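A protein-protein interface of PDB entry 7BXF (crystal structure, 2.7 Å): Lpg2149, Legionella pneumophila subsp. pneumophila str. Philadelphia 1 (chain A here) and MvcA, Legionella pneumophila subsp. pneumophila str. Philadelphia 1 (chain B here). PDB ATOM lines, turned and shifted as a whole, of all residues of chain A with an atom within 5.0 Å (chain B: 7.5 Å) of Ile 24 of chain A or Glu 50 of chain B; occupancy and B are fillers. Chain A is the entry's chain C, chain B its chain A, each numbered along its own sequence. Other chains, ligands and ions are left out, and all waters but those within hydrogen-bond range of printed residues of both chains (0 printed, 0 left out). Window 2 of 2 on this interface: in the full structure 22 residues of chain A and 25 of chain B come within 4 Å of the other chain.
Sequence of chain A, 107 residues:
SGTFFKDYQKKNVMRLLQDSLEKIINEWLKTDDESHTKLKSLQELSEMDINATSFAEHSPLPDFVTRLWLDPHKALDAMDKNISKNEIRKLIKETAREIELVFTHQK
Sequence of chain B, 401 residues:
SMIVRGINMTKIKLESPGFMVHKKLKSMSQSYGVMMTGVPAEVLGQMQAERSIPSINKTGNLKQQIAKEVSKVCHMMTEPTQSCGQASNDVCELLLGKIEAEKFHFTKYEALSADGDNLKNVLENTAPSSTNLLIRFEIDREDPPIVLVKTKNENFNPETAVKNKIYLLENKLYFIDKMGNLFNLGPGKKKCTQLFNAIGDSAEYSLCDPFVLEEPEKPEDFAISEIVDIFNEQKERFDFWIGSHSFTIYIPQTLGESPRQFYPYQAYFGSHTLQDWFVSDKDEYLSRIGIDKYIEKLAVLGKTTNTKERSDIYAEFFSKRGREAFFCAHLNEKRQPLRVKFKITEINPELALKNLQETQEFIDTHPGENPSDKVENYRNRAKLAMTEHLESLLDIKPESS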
ATOM      1  N   SER A  20     -32.294   2.177  13.258  1.00  0.00           N
ATOM      2  CA  SER A  20     -31.493   1.372  12.344  1.00  0.00           C
ATOM      3  C   SER A  20     -30.506   2.237  11.580  1.00  0.00           C
ATOM      4  O   SER A  20     -29.367   1.822  11.339  1.00  0.00           O
ATOM      5  CB  SER A  20     -32.408   0.622  11.379  1.00  0.00           C
ATOM      6  OG  SER A  20     -33.463  -0.010  12.086  1.00  0.00           O
ATOM      7  N   LEU A  21     -30.924   3.442  11.187  1.00  0.00           N
ATOM      8  CA  LEU A  21     -30.001   4.371  10.545  1.00  0.00           C
ATOM      9  C   LEU A  21     -28.847   4.715  11.477  1.00  0.00           C
ATOM     10  O   LEU A  21     -27.677   4.682  11.076  1.00  0.00           O
ATOM     11  CB  LEU A  21     -30.742   5.633  10.118  1.00  0.00           C
ATOM     12  CG  LEU A  21     -31.600   5.501   8.860  1.00  0.00           C
ATOM     13  CD1 LEU A  21     -32.290   6.820   8.576  1.00  0.00           C
ATOM     14  CD2 LEU A  21     -30.746   5.064   7.682  1.00  0.00           C
ATOM     15  N   GLU A  22     -29.162   5.030  12.735  1.00  0.00           N
ATOM     16  CA  GLU A  22     -28.123   5.400  13.690  1.00  0.00           C
ATOM     17  C   GLU A  22     -27.137   4.260  13.908  1.00  0.00           C
ATOM     18  O   GLU A  22     -25.922   4.484  13.942  1.00  0.00           O
ATOM     19  CB  GLU A  22     -28.757   5.828  15.014  1.00  0.00           C
ATOM     20  CG  GLU A  22     -28.993   7.328  15.128  1.00  0.00           C
ATOM     21  CD  GLU A  22     -30.108   7.687  16.093  1.00  0.00           C
ATOM     22  OE1 GLU A  22     -30.696   6.768  16.700  1.00  0.00           O
ATOM     23  OE2 GLU A  22     -30.403   8.894  16.237  1.00  0.00           O
ATOM     24  N   LYS A  23     -27.635   3.029  14.039  1.00  0.00           N
ATOM     25  CA  LYS A  23     -26.737   1.909  14.302  1.00  0.00           C
ATOM     26  C   LYS A  23     -25.844   1.619  13.101  1.00  0.00           C
ATOM     27  O   LYS A  23     -24.649   1.337  13.261  1.00  0.00           O
ATOM     28  CB  LYS A  23     -27.538   0.666  14.694  1.00  0.00           C
ATOM     29  CG  LYS A  23     -27.447   0.325  16.181  1.00  0.00           C
ATOM     30  CD  LYS A  23     -27.904  -1.100  16.459  1.00  0.00           C
ATOM     31  CE  LYS A  23     -27.307  -2.080  15.453  1.00  0.00           C
ATOM     32  NZ  LYS A  23     -27.903  -3.442  15.567  1.00  0.00           N
ATOM     33  N   ILE A  24     -26.400   1.701  11.893  1.00  0.00           N
ATOM     34  CA  ILE A  24     -25.628   1.382  10.696  1.00  0.00           C
ATOM     35  C   ILE A  24     -24.601   2.475  10.412  1.00  0.00           C
ATOM     36  O   ILE A  24     -23.426   2.192  10.143  1.00  0.00           O
ATOM     37  CB  ILE A  24     -26.577   1.160   9.505  1.00  0.00           C
ATOM     38  CG1 ILE A  24     -27.481  -0.049   9.767  1.00  0.00           C
ATOM     39  CG2 ILE A  24     -25.795   0.981   8.218  1.00  0.00           C
ATOM     40  CD1 ILE A  24     -28.569  -0.224   8.728  1.00  0.00           C
ATOM     41  N   ILE A  25     -25.027   3.740  10.473  1.00  0.00           N
ATOM     42  CA  ILE A  25     -24.112   4.851  10.220  1.00  0.00           C
ATOM     43  C   ILE A  25     -22.987   4.866  11.248  1.00  0.00           C
ATOM     44  O   ILE A  25     -21.824   5.125  10.913  1.00  0.00           O
ATOM     45  CB  ILE A  25     -24.884   6.184  10.207  1.00  0.00           C
ATOM     46  CG1 ILE A  25     -25.929   6.190   9.090  1.00  0.00           C
ATOM     47  CG2 ILE A  25     -23.932   7.362  10.060  1.00  0.00           C
ATOM     48  CD1 ILE A  25     -26.845   7.390   9.135  1.00  0.00           C
ATOM     49  N   ASN A  26     -23.311   4.586  12.512  1.00  0.00           N
ATOM     50  CA  ASN A  26     -22.293   4.611  13.561  1.00  0.00           C
ATOM     51  C   ASN A  26     -21.260   3.511  13.355  1.00  0.00           C
ATOM     52  O   ASN A  26     -20.053   3.752  13.482  1.00  0.00           O
ATOM     53  CB  ASN A  26     -22.944   4.482  14.939  1.00  0.00           C
ATOM     54  CG  ASN A  26     -23.575   5.775  15.404  1.00  0.00           C
ATOM     55  OD1 ASN A  26     -23.160   6.858  14.997  1.00  0.00           O
ATOM     56  ND2 ASN A  26     -24.588   5.669  16.254  1.00  0.00           N
ATOM     57  N   GLU A  27     -21.714   2.292  13.052  1.00  0.00           N
ATOM     58  CA  GLU A  27     -20.770   1.223  12.741  1.00  0.00           C
ATOM     59  C   GLU A  27     -19.902   1.604  11.550  1.00  0.00           C
ATOM     60  O   GLU A  27     -18.692   1.346  11.539  1.00  0.00           O
ATOM     61  CB  GLU A  27     -21.526  -0.080  12.474  1.00  0.00           C
ATOM     62  CG  GLU A  27     -20.660  -1.336  12.480  1.00  0.00           C
ATOM     63  CD  GLU A  27     -19.790  -1.447  13.722  1.00  0.00           C
ATOM     64  OE1 GLU A  27     -18.595  -1.802  13.591  1.00  0.00           O
ATOM     65  OE2 GLU A  27     -20.305  -1.185  14.831  1.00  0.00           O
ATOM     66  N   TRP A  28     -20.503   2.253  10.552  1.00  0.00           N
ATOM     67  CA  TRP A  28     -19.757   2.708   9.386  1.00  0.00           C
ATOM     68  C   TRP A  28     -18.832   3.873   9.726  1.00  0.00           C
ATOM     69  O   TRP A  28     -17.752   3.998   9.139  1.00  0.00           O
ATOM     70  CB  TRP A  28     -20.746   3.080   8.284  1.00  0.00           C
ATOM     71  CG  TRP A  28     -20.207   3.903   7.162  1.00  0.00           C
ATOM     72  CD1 TRP A  28     -19.453   3.468   6.111  1.00  0.00           C
ATOM     73  CD2 TRP A  28     -20.415   5.305   6.953  1.00  0.00           C
ATOM     74  NE1 TRP A  28     -19.169   4.514   5.268  1.00  0.00           N
ATOM     75  CE2 TRP A  28     -19.748   5.654   5.762  1.00  0.00           C
ATOM     76  CE3 TRP A  28     -21.099   6.302   7.662  1.00  0.00           C
ATOM     77  CZ2 TRP A  28     -19.743   6.956   5.261  1.00  0.00           C
ATOM     78  CZ3 TRP A  28     -21.090   7.596   7.166  1.00  0.00           C
ATOM     79  CH2 TRP A  28     -20.415   7.912   5.976  1.00  0.00           C
ATOM     80  N   LEU A  29     -19.227   4.725  10.677  1.00  0.00           N
ATOM     81  CA  LEU A  29     -18.367   5.835  11.080  1.00  0.00           C
ATOM     82  C   LEU A  29     -17.168   5.359  11.896  1.00  0.00           C
ATOM     83  O   LEU A  29     -16.110   5.997  11.870  1.00  0.00           O
ATOM     84  CB  LEU A  29     -19.181   6.861  11.869  1.00  0.00           C
ATOM     85  CG  LEU A  29     -19.022   8.337  11.503  1.00  0.00           C
ATOM     86  CD1 LEU A  29     -18.876   8.521  10.001  1.00  0.00           C
ATOM     87  CD2 LEU A  29     -20.212   9.122  12.017  1.00  0.00           C
ATOM     88  N   PRO A  62     -23.333   4.686   3.283  1.00  0.00           N
ATOM     89  CA  PRO A  62     -23.705   3.269   3.353  1.00  0.00           C
ATOM     90  C   PRO A  62     -24.787   2.924   2.343  1.00  0.00           C
ATOM     91  O   PRO A  62     -25.653   3.741   2.021  1.00  0.00           O
ATOM     92  CB  PRO A  62     -24.209   3.104   4.792  1.00  0.00           C
ATOM     93  CG  PRO A  62     -23.575   4.234   5.545  1.00  0.00           C
ATOM     94  CD  PRO A  62     -23.545   5.371   4.569  1.00  0.00           C
ATOM     95  N   PHE A  64     -27.447   1.160   2.470  1.00  0.00           N
ATOM     96  CA  PHE A  64     -28.832   1.307   2.913  1.00  0.00           C
ATOM     97  C   PHE A  64     -29.287   2.759   2.810  1.00  0.00           C
ATOM     98  O   PHE A  64     -30.379   3.043   2.300  1.00  0.00           O
ATOM     99  CB  PHE A  64     -28.986   0.784   4.347  1.00  0.00           C
ATOM    100  CG  PHE A  64     -30.338   1.054   4.961  1.00  0.00           C
ATOM    101  CD1 PHE A  64     -31.511   0.814   4.251  1.00  0.00           C
ATOM    102  CD2 PHE A  64     -30.437   1.547   6.256  1.00  0.00           C
ATOM    103  CE1 PHE A  64     -32.756   1.068   4.818  1.00  0.00           C
ATOM    104  CE2 PHE A  64     -31.679   1.800   6.830  1.00  0.00           C
ATOM    105  CZ  PHE A  64     -32.838   1.559   6.107  1.00  0.00           C
ATOM    106  N   ARG A  67     -29.868   3.674  -0.850  1.00  0.00           N
ATOM    107  CA  ARG A  67     -31.036   2.946  -1.340  1.00  0.00           C
ATOM    108  C   ARG A  67     -32.314   3.492  -0.724  1.00  0.00           C
ATOM    109  O   ARG A  67     -33.326   3.660  -1.416  1.00  0.00           O
ATOM    110  CB  ARG A  67     -30.909   1.455  -1.030  1.00  0.00           C
ATOM    111  CG  ARG A  67     -30.173   0.634  -2.071  1.00  0.00           C
ATOM    112  CD  ARG A  67     -30.316  -0.854  -1.770  1.00  0.00           C
ATOM    113  NE  ARG A  67     -29.632  -1.228  -0.532  1.00  0.00           N
ATOM    114  CZ  ARG A  67     -30.250  -1.476   0.620  1.00  0.00           C
ATOM    115  NH1 ARG A  67     -31.573  -1.395   0.702  1.00  0.00           N
ATOM    116  NH2 ARG A  67     -29.542  -1.806   1.694  1.00  0.00           N
ATOM    117  N   ALA A  75     -36.598  -0.115  -1.148  1.00  0.00           N
ATOM    118  CA  ALA A  75     -35.606  -0.464  -0.137  1.00  0.00           C
ATOM    119  C   ALA A  75     -36.235  -1.248   1.005  1.00  0.00           C
ATOM    120  O   ALA A  75     -35.635  -2.199   1.518  1.00  0.00           O
ATOM    121  CB  ALA A  75     -34.930   0.800   0.393  1.00  0.00           C
ATOM    122  N   LEU A  76     -37.442  -0.855   1.423  1.00  0.00           N
ATOM    123  CA  LEU A  76     -38.198  -1.540   2.476  1.00  0.00           C
ATOM    124  C   LEU A  76     -39.627  -1.722   1.967  1.00  0.00           C
ATOM    125  O   LEU A  76     -40.514  -0.913   2.258  1.00  0.00           O
ATOM    126  CB  LEU A  76     -38.151  -0.755   3.781  1.00  0.00           C
ATOM    127  CG  LEU A  76     -36.772  -0.612   4.427  1.00  0.00           C
ATOM    128  CD1 LEU A  76     -36.830   0.423   5.530  1.00  0.00           C
ATOM    129  CD2 LEU A  76     -36.269  -1.958   4.963  1.00  0.00           C
ATOM    130  N   LEU B  44     -40.361  -5.051  10.685  1.00  0.00           N
ATOM    131  CA  LEU B  44     -39.324  -5.230  11.698  1.00  0.00           C
ATOM    132  C   LEU B  44     -38.259  -6.218  11.239  1.00  0.00           C
ATOM    133  O   LEU B  44     -37.062  -6.008  11.478  1.00  0.00           O
ATOM    134  CB  LEU B  44     -39.952  -5.682  13.016  1.00  0.00           C
ATOM    135  CG  LEU B  44     -38.989  -6.276  14.044  1.00  0.00           C
ATOM    136  CD1 LEU B  44     -38.140  -5.167  14.656  1.00  0.00           C
ATOM    137  CD2 LEU B  44     -39.725  -7.071  15.120  1.00  0.00           C
ATOM    138  N   GLY B  45     -38.670  -7.303  10.581  1.00  0.00           N
ATOM    139  CA  GLY B  45     -37.695  -8.243  10.054  1.00  0.00           C
ATOM    140  C   GLY B  45     -36.861  -7.648   8.936  1.00  0.00           C
ATOM    141  O   GLY B  45     -35.647  -7.852   8.879  1.00  0.00           O
ATOM    142  N   GLN B  46     -37.501  -6.897   8.037  1.00  0.00           N
ATOM    143  CA  GLN B  46     -36.775  -6.268   6.938  1.00  0.00           C
ATOM    144  C   GLN B  46     -35.673  -5.352   7.452  1.00  0.00           C
ATOM    145  O   GLN B  46     -34.590  -5.271   6.861  1.00  0.00           O
ATOM    146  CB  GLN B  46     -37.746  -5.479   6.064  1.00  0.00           C
ATOM    147  CG  GLN B  46     -38.320  -6.242   4.898  1.00  0.00           C
ATOM    148  CD  GLN B  46     -39.270  -5.388   4.101  1.00  0.00           C
ATOM    149  OE1 GLN B  46     -39.609  -4.273   4.513  1.00  0.00           O
ATOM    150  NE2 GLN B  46     -39.712  -5.899   2.960  1.00  0.00           N
ATOM    151  N   MET B  47     -36.010  -4.592   8.500  1.00  0.00           N
ATOM    152  CA  MET B  47     -35.079  -3.615   9.127  1.00  0.00           C
ATOM    153  C   MET B  47     -33.916  -4.378   9.763  1.00  0.00           C
ATOM    154  O   MET B  47     -32.753  -4.025   9.481  1.00  0.00           O
ATOM    155  CB  MET B  47     -35.795  -2.793  10.203  1.00  0.00           C
ATOM    156  CG  MET B  47     -35.703  -1.296   9.982  1.00  0.00           C
ATOM    157  SD  MET B  47     -37.168  -0.414  10.577  1.00  0.00           S
ATOM    158  CE  MET B  47     -37.934   0.038   9.022  1.00  0.00           C
ATOM    159  N   GLN B  48     -34.231  -5.377  10.593  1.00  0.00           N
ATOM    160  CA  GLN B  48     -33.198  -6.177  11.237  1.00  0.00           C
ATOM    161  C   GLN B  48     -32.222  -6.718  10.207  1.00  0.00           C
ATOM    162  O   GLN B  48     -31.008  -6.760  10.451  1.00  0.00           O
ATOM    163  CB  GLN B  48     -33.833  -7.316  12.032  1.00  0.00           C
ATOM    164  CG  GLN B  48     -34.281  -6.880  13.409  1.00  0.00           C
ATOM    165  CD  GLN B  48     -35.256  -7.847  14.046  1.00  0.00           C
ATOM    166  OE1 GLN B  48     -35.886  -8.656  13.364  1.00  0.00           O
ATOM    167  NE2 GLN B  48     -35.402  -7.753  15.364  1.00  0.00           N
ATOM    168  N   ALA B  49     -32.736  -7.113   9.038  1.00  0.00           N
ATOM    169  CA  ALA B  49     -31.862  -7.525   7.946  1.00  0.00           C
ATOM    170  C   ALA B  49     -30.947  -6.384   7.519  1.00  0.00           C
ATOM    171  O   ALA B  49     -29.787  -6.612   7.162  1.00  0.00           O
ATOM    172  CB  ALA B  49     -32.700  -8.027   6.768  1.00  0.00           C
ATOM    173  N   GLU B  50     -31.445  -5.145   7.575  1.00  0.00           N
ATOM    174  CA  GLU B  50     -30.651  -3.998   7.146  1.00  0.00           C
ATOM    175  C   GLU B  50     -29.534  -3.688   8.134  1.00  0.00           C
ATOM    176  O   GLU B  50     -28.397  -3.414   7.729  1.00  0.00           O
ATOM    177  CB  GLU B  50     -31.543  -2.769   6.960  1.00  0.00           C
ATOM    178  CG  GLU B  50     -32.424  -2.791   5.718  1.00  0.00           C
ATOM    179  CD  GLU B  50     -31.646  -2.759   4.412  1.00  0.00           C
ATOM    180  OE1 GLU B  50     -30.402  -2.636   4.441  1.00  0.00           O
ATOM    181  OE2 GLU B  50     -32.291  -2.847   3.343  1.00  0.00           O
ATOM    182  N   ARG B  51     -29.833  -3.700   9.430  1.00  0.00           N
ATOM    183  CA  ARG B  51     -28.787  -3.448  10.409  1.00  0.00           C
ATOM    184  C   ARG B  51     -27.888  -4.656  10.626  1.00  0.00           C
ATOM    185  O   ARG B  51     -26.945  -4.568  11.420  1.00  0.00           O
ATOM    186  CB  ARG B  51     -29.391  -3.000  11.743  1.00  0.00           C
ATOM    187  CG  ARG B  51     -30.736  -3.601  12.041  1.00  0.00           C
ATOM    188  CD  ARG B  51     -31.485  -2.801  13.079  1.00  0.00           C
ATOM    189  NE  ARG B  51     -31.037  -3.176  14.411  1.00  0.00           N
ATOM    190  CZ  ARG B  51     -31.225  -2.440  15.497  1.00  0.00           C
ATOM    191  NH1 ARG B  51     -31.864  -1.279  15.410  1.00  0.00           N
ATOM    192  NH2 ARG B  51     -30.773  -2.874  16.669  1.00  0.00           N
ATOM    193  N   SER B  52     -28.140  -5.771   9.936  1.00  0.00           N
ATOM    194  CA  SER B  52     -27.285  -6.946  10.031  1.00  0.00           C
ATOM    195  C   SER B  52     -26.508  -7.241   8.754  1.00  0.00           C
ATOM    196  O   SER B  52     -25.662  -8.140   8.761  1.00  0.00           O
ATOM    197  CB  SER B  52     -28.111  -8.188  10.409  1.00  0.00           C
ATOM    198  OG  SER B  52     -28.409  -8.951   9.256  1.00  0.00           O
ATOM    199  N   ILE B  53     -26.758  -6.514   7.669  1.00  0.00           N
ATOM    200  CA  ILE B  53     -26.102  -6.801   6.393  1.00  0.00           C
ATOM    201  C   ILE B  53     -24.692  -6.200   6.298  1.00  0.00           C
ATOM    202  O   ILE B  53     -23.890  -6.697   5.493  1.00  0.00           O
ATOM    203  CB  ILE B  53     -26.988  -6.357   5.211  1.00  0.00           C
ATOM    204  CG1 ILE B  53     -26.461  -6.934   3.889  1.00  0.00           C
ATOM    205  CG2 ILE B  53     -27.101  -4.843   5.135  1.00  0.00           C
ATOM    206  CD1 ILE B  53     -27.222  -6.492   2.657  1.00  0.00           C
ATOM    207  N   PRO B  54     -24.304  -5.183   7.083  1.00  0.00           N
ATOM    208  CA  PRO B  54     -22.872  -4.830   7.078  1.00  0.00           C
ATOM    209  C   PRO B  54     -21.981  -5.949   7.588  1.00  0.00           C
ATOM    210  O   PRO B  54     -20.880  -6.148   7.057  1.00  0.00           O
ATOM    211  CB  PRO B  54     -22.812  -3.589   7.980  1.00  0.00           C
ATOM    212  CG  PRO B  54     -24.165  -3.003   7.894  1.00  0.00           C
ATOM    213  CD  PRO B  54     -25.080  -4.181   7.845  1.00  0.00           C
ATOM    214  N   SER B  55     -22.430  -6.699   8.600  1.00  0.00           N
ATOM    215  CA  SER B  55     -21.631  -7.770   9.187  1.00  0.00           C
ATOM    216  C   SER B  55     -21.486  -8.980   8.274  1.00  0.00           C
ATOM    217  O   SER B  55     -20.811  -9.942   8.656  1.00  0.00           O
ATOM    218  CB  SER B  55     -22.242  -8.215  10.518  1.00  0.00           C
ATOM    219  OG  SER B  55     -22.433  -7.119  11.397  1.00  0.00           O
ATOM    220  N   MET B 386     -37.032 -11.079   7.469  1.00  0.00           N
ATOM    221  CA  MET B 386     -35.586 -10.786   7.661  1.00  0.00           C
ATOM    222  C   MET B 386     -34.767 -11.672   6.715  1.00  0.00           C
ATOM    223  O   MET B 386     -33.761 -11.180   6.166  1.00  0.00           O
ATOM    224  CB  MET B 386     -35.161 -11.058   9.107  1.00  0.00           C
ATOM    225  CG  MET B 386     -33.677 -11.336   9.260  1.00  0.00           C
ATOM    226  SD  MET B 386     -33.030 -10.798  10.863  1.00  0.00           S
ATOM    227  CE  MET B 386     -33.200 -12.309  11.811  1.00  0.00           C
ATOM    228  N   HIS B 389     -35.449 -10.527   2.969  1.00  0.00           N
ATOM    229  CA  HIS B 389     -34.827  -9.243   2.672  1.00  0.00           C
ATOM    230  C   HIS B 389     -33.318  -9.370   2.588  1.00  0.00           C
ATOM    231  O   HIS B 389     -32.670  -8.639   1.826  1.00  0.00           O
ATOM    232  CB  HIS B 389     -35.217  -8.216   3.730  1.00  0.00           C
ATOM    233  CG  HIS B 389     -34.910  -6.808   3.340  1.00  0.00           C
ATOM    234  ND1 HIS B 389     -35.579  -6.158   2.327  1.00  0.00           N
ATOM    235  CD2 HIS B 389     -34.011  -5.921   3.828  1.00  0.00           C
ATOM    236  CE1 HIS B 389     -35.101  -4.934   2.201  1.00  0.00           C
ATOM    237  NE2 HIS B 389     -34.151  -4.763   3.103  1.00  0.00           N
ATOM    238  N   LEU B 390     -32.745 -10.288   3.366  1.00  0.00           N
ATOM    239  CA  LEU B 390     -31.327 -10.594   3.241  1.00  0.00           C
ATOM    240  C   LEU B 390     -31.029 -11.225   1.883  1.00  0.00           C
ATOM    241  O   LEU B 390     -30.001 -10.925   1.263  1.00  0.00           O
ATOM    242  CB  LEU B 390     -30.910 -11.514   4.391  1.00  0.00           C
ATOM    243  CG  LEU B 390     -29.685 -11.159   5.232  1.00  0.00           C
ATOM    244  CD1 LEU B 390     -29.712  -9.695   5.604  1.00  0.00           C
ATOM    245  CD2 LEU B 390     -29.634 -12.033   6.486  1.00  0.00           C
ATOM    246  N   SER B 392     -32.782 -10.952  -1.040  1.00  0.00           N
ATOM    247  CA  SER B 392     -32.952 -10.038  -2.163  1.00  0.00           C
ATOM    248  C   SER B 392     -31.788  -9.066  -2.292  1.00  0.00           C
ATOM    249  O   SER B 392     -31.551  -8.543  -3.386  1.00  0.00           O
ATOM    250  CB  SER B 392     -34.267  -9.268  -2.025  1.00  0.00           C
ATOM    251  OG  SER B 392     -34.219  -8.362  -0.938  1.00  0.00           O
ATOM    252  N   LEU B 393     -31.056  -8.821  -1.204  1.00  0.00           N
ATOM    253  CA  LEU B 393     -29.919  -7.915  -1.218  1.00  0.00           C
ATOM    254  C   LEU B 393     -28.607  -8.606  -1.560  1.00  0.00           C
ATOM    255  O   LEU B 393     -27.673  -7.939  -2.020  1.00  0.00           O
ATOM    256  CB  LEU B 393     -29.793  -7.217   0.140  1.00  0.00           C
ATOM    257  CG  LEU B 393     -30.926  -6.226   0.429  1.00  0.00           C
ATOM    258  CD1 LEU B 393     -30.817  -5.641   1.831  1.00  0.00           C
ATOM    259  CD2 LEU B 393     -30.950  -5.121  -0.617  1.00  0.00           C
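Printed residues of chain B that touch a printed residue of chain A: Gln 46, Met 47, Glu 50, Arg 51, His 389 and Leu 393.
Hydrophobic or aromatic side chains of chain B within 4 Å of the printed part of chain A: Met 47, His 389 and Leu 393.
Hydrophobic or aromatic side chains of chain A within 4 Å of the printed part of chain B: Ile 24, Phe 64 and Leu 76.
Among the printed residues, 13 pairs touch across the chains.
NH2 of Arg 67 of chain A lies within salt-bridge range of OE1 of Glu 50 of chain B (3.0 Å).
A ring nitrogen (NE2) of His 389 of chain B sits close to the backbone carbonyl oxygen (O) of Ala 75 of chain A (3.4 Å).
The guanidinium group of Arg 51 of chain B lies close to the side-chain amino group of Lys 23 of chain A.
Among the printed residues, merely in contact across the chains: Ser 20 of chain A with Met 47 of chain B (3.3 Å), Ile 24 of chain A with Glu 50 of chain B (3.3 Å), Ser 20 of chain A with Arg 51 of chain B (3.6 Å), Phe 64 of chain A with Glu 50 of chain B (3.6 Å), Leu 76 of chain A with Gln 46 of chain B (3.6 Å), Ile 24 of chain A with Arg 51 of chain B (3.6 Å), Leu 76 of chain A with Met 47 of chain B (3.7 Å), Ala 75 of chain A with Glu 50 of chain B (3.9 Å), Arg 67 of chain A with Leu 393 of chain B (3.9 Å) and Leu 76 of chain A with His 389 of chain B (3.98 Å).
The side-chain carboxylate (OE2) of Glu 50 of chain B lies within hydrogen-bond range of a ring nitrogen (NE2) of His 389 of chain B, at 2.7 Å.
OG of Ser 392 of chain B lies within hydrogen-bond range of O of His 389 of chain B (3.2 Å).
Of the printed residues of chain B, Lys 23 of chain A touches Arg 51.
Ile 24 of chain A touches two residues of chain B.
Ile 25 of chain A touches none of the printed residues of chain B.
Printed residues of chain B within 4 Å of Leu 76 of chain A: Gln 46, Met 47 and His 389.
Of the printed residues of chain A, Glu 50 of chain B touches Ile 24 (3.3 Å), Phe 64 (3.6 Å), Arg 67 (3.0 Å) and Ala 75 (3.9 Å).
Printed residues of chain A within 4 Å of Arg 51 of chain B: Ser 20 (3.6 Å), Lys 23 (3.1 Å) and Ile 24 (3.6 Å).
Pro 54 of chain B touches none of the printed residues of chain A.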
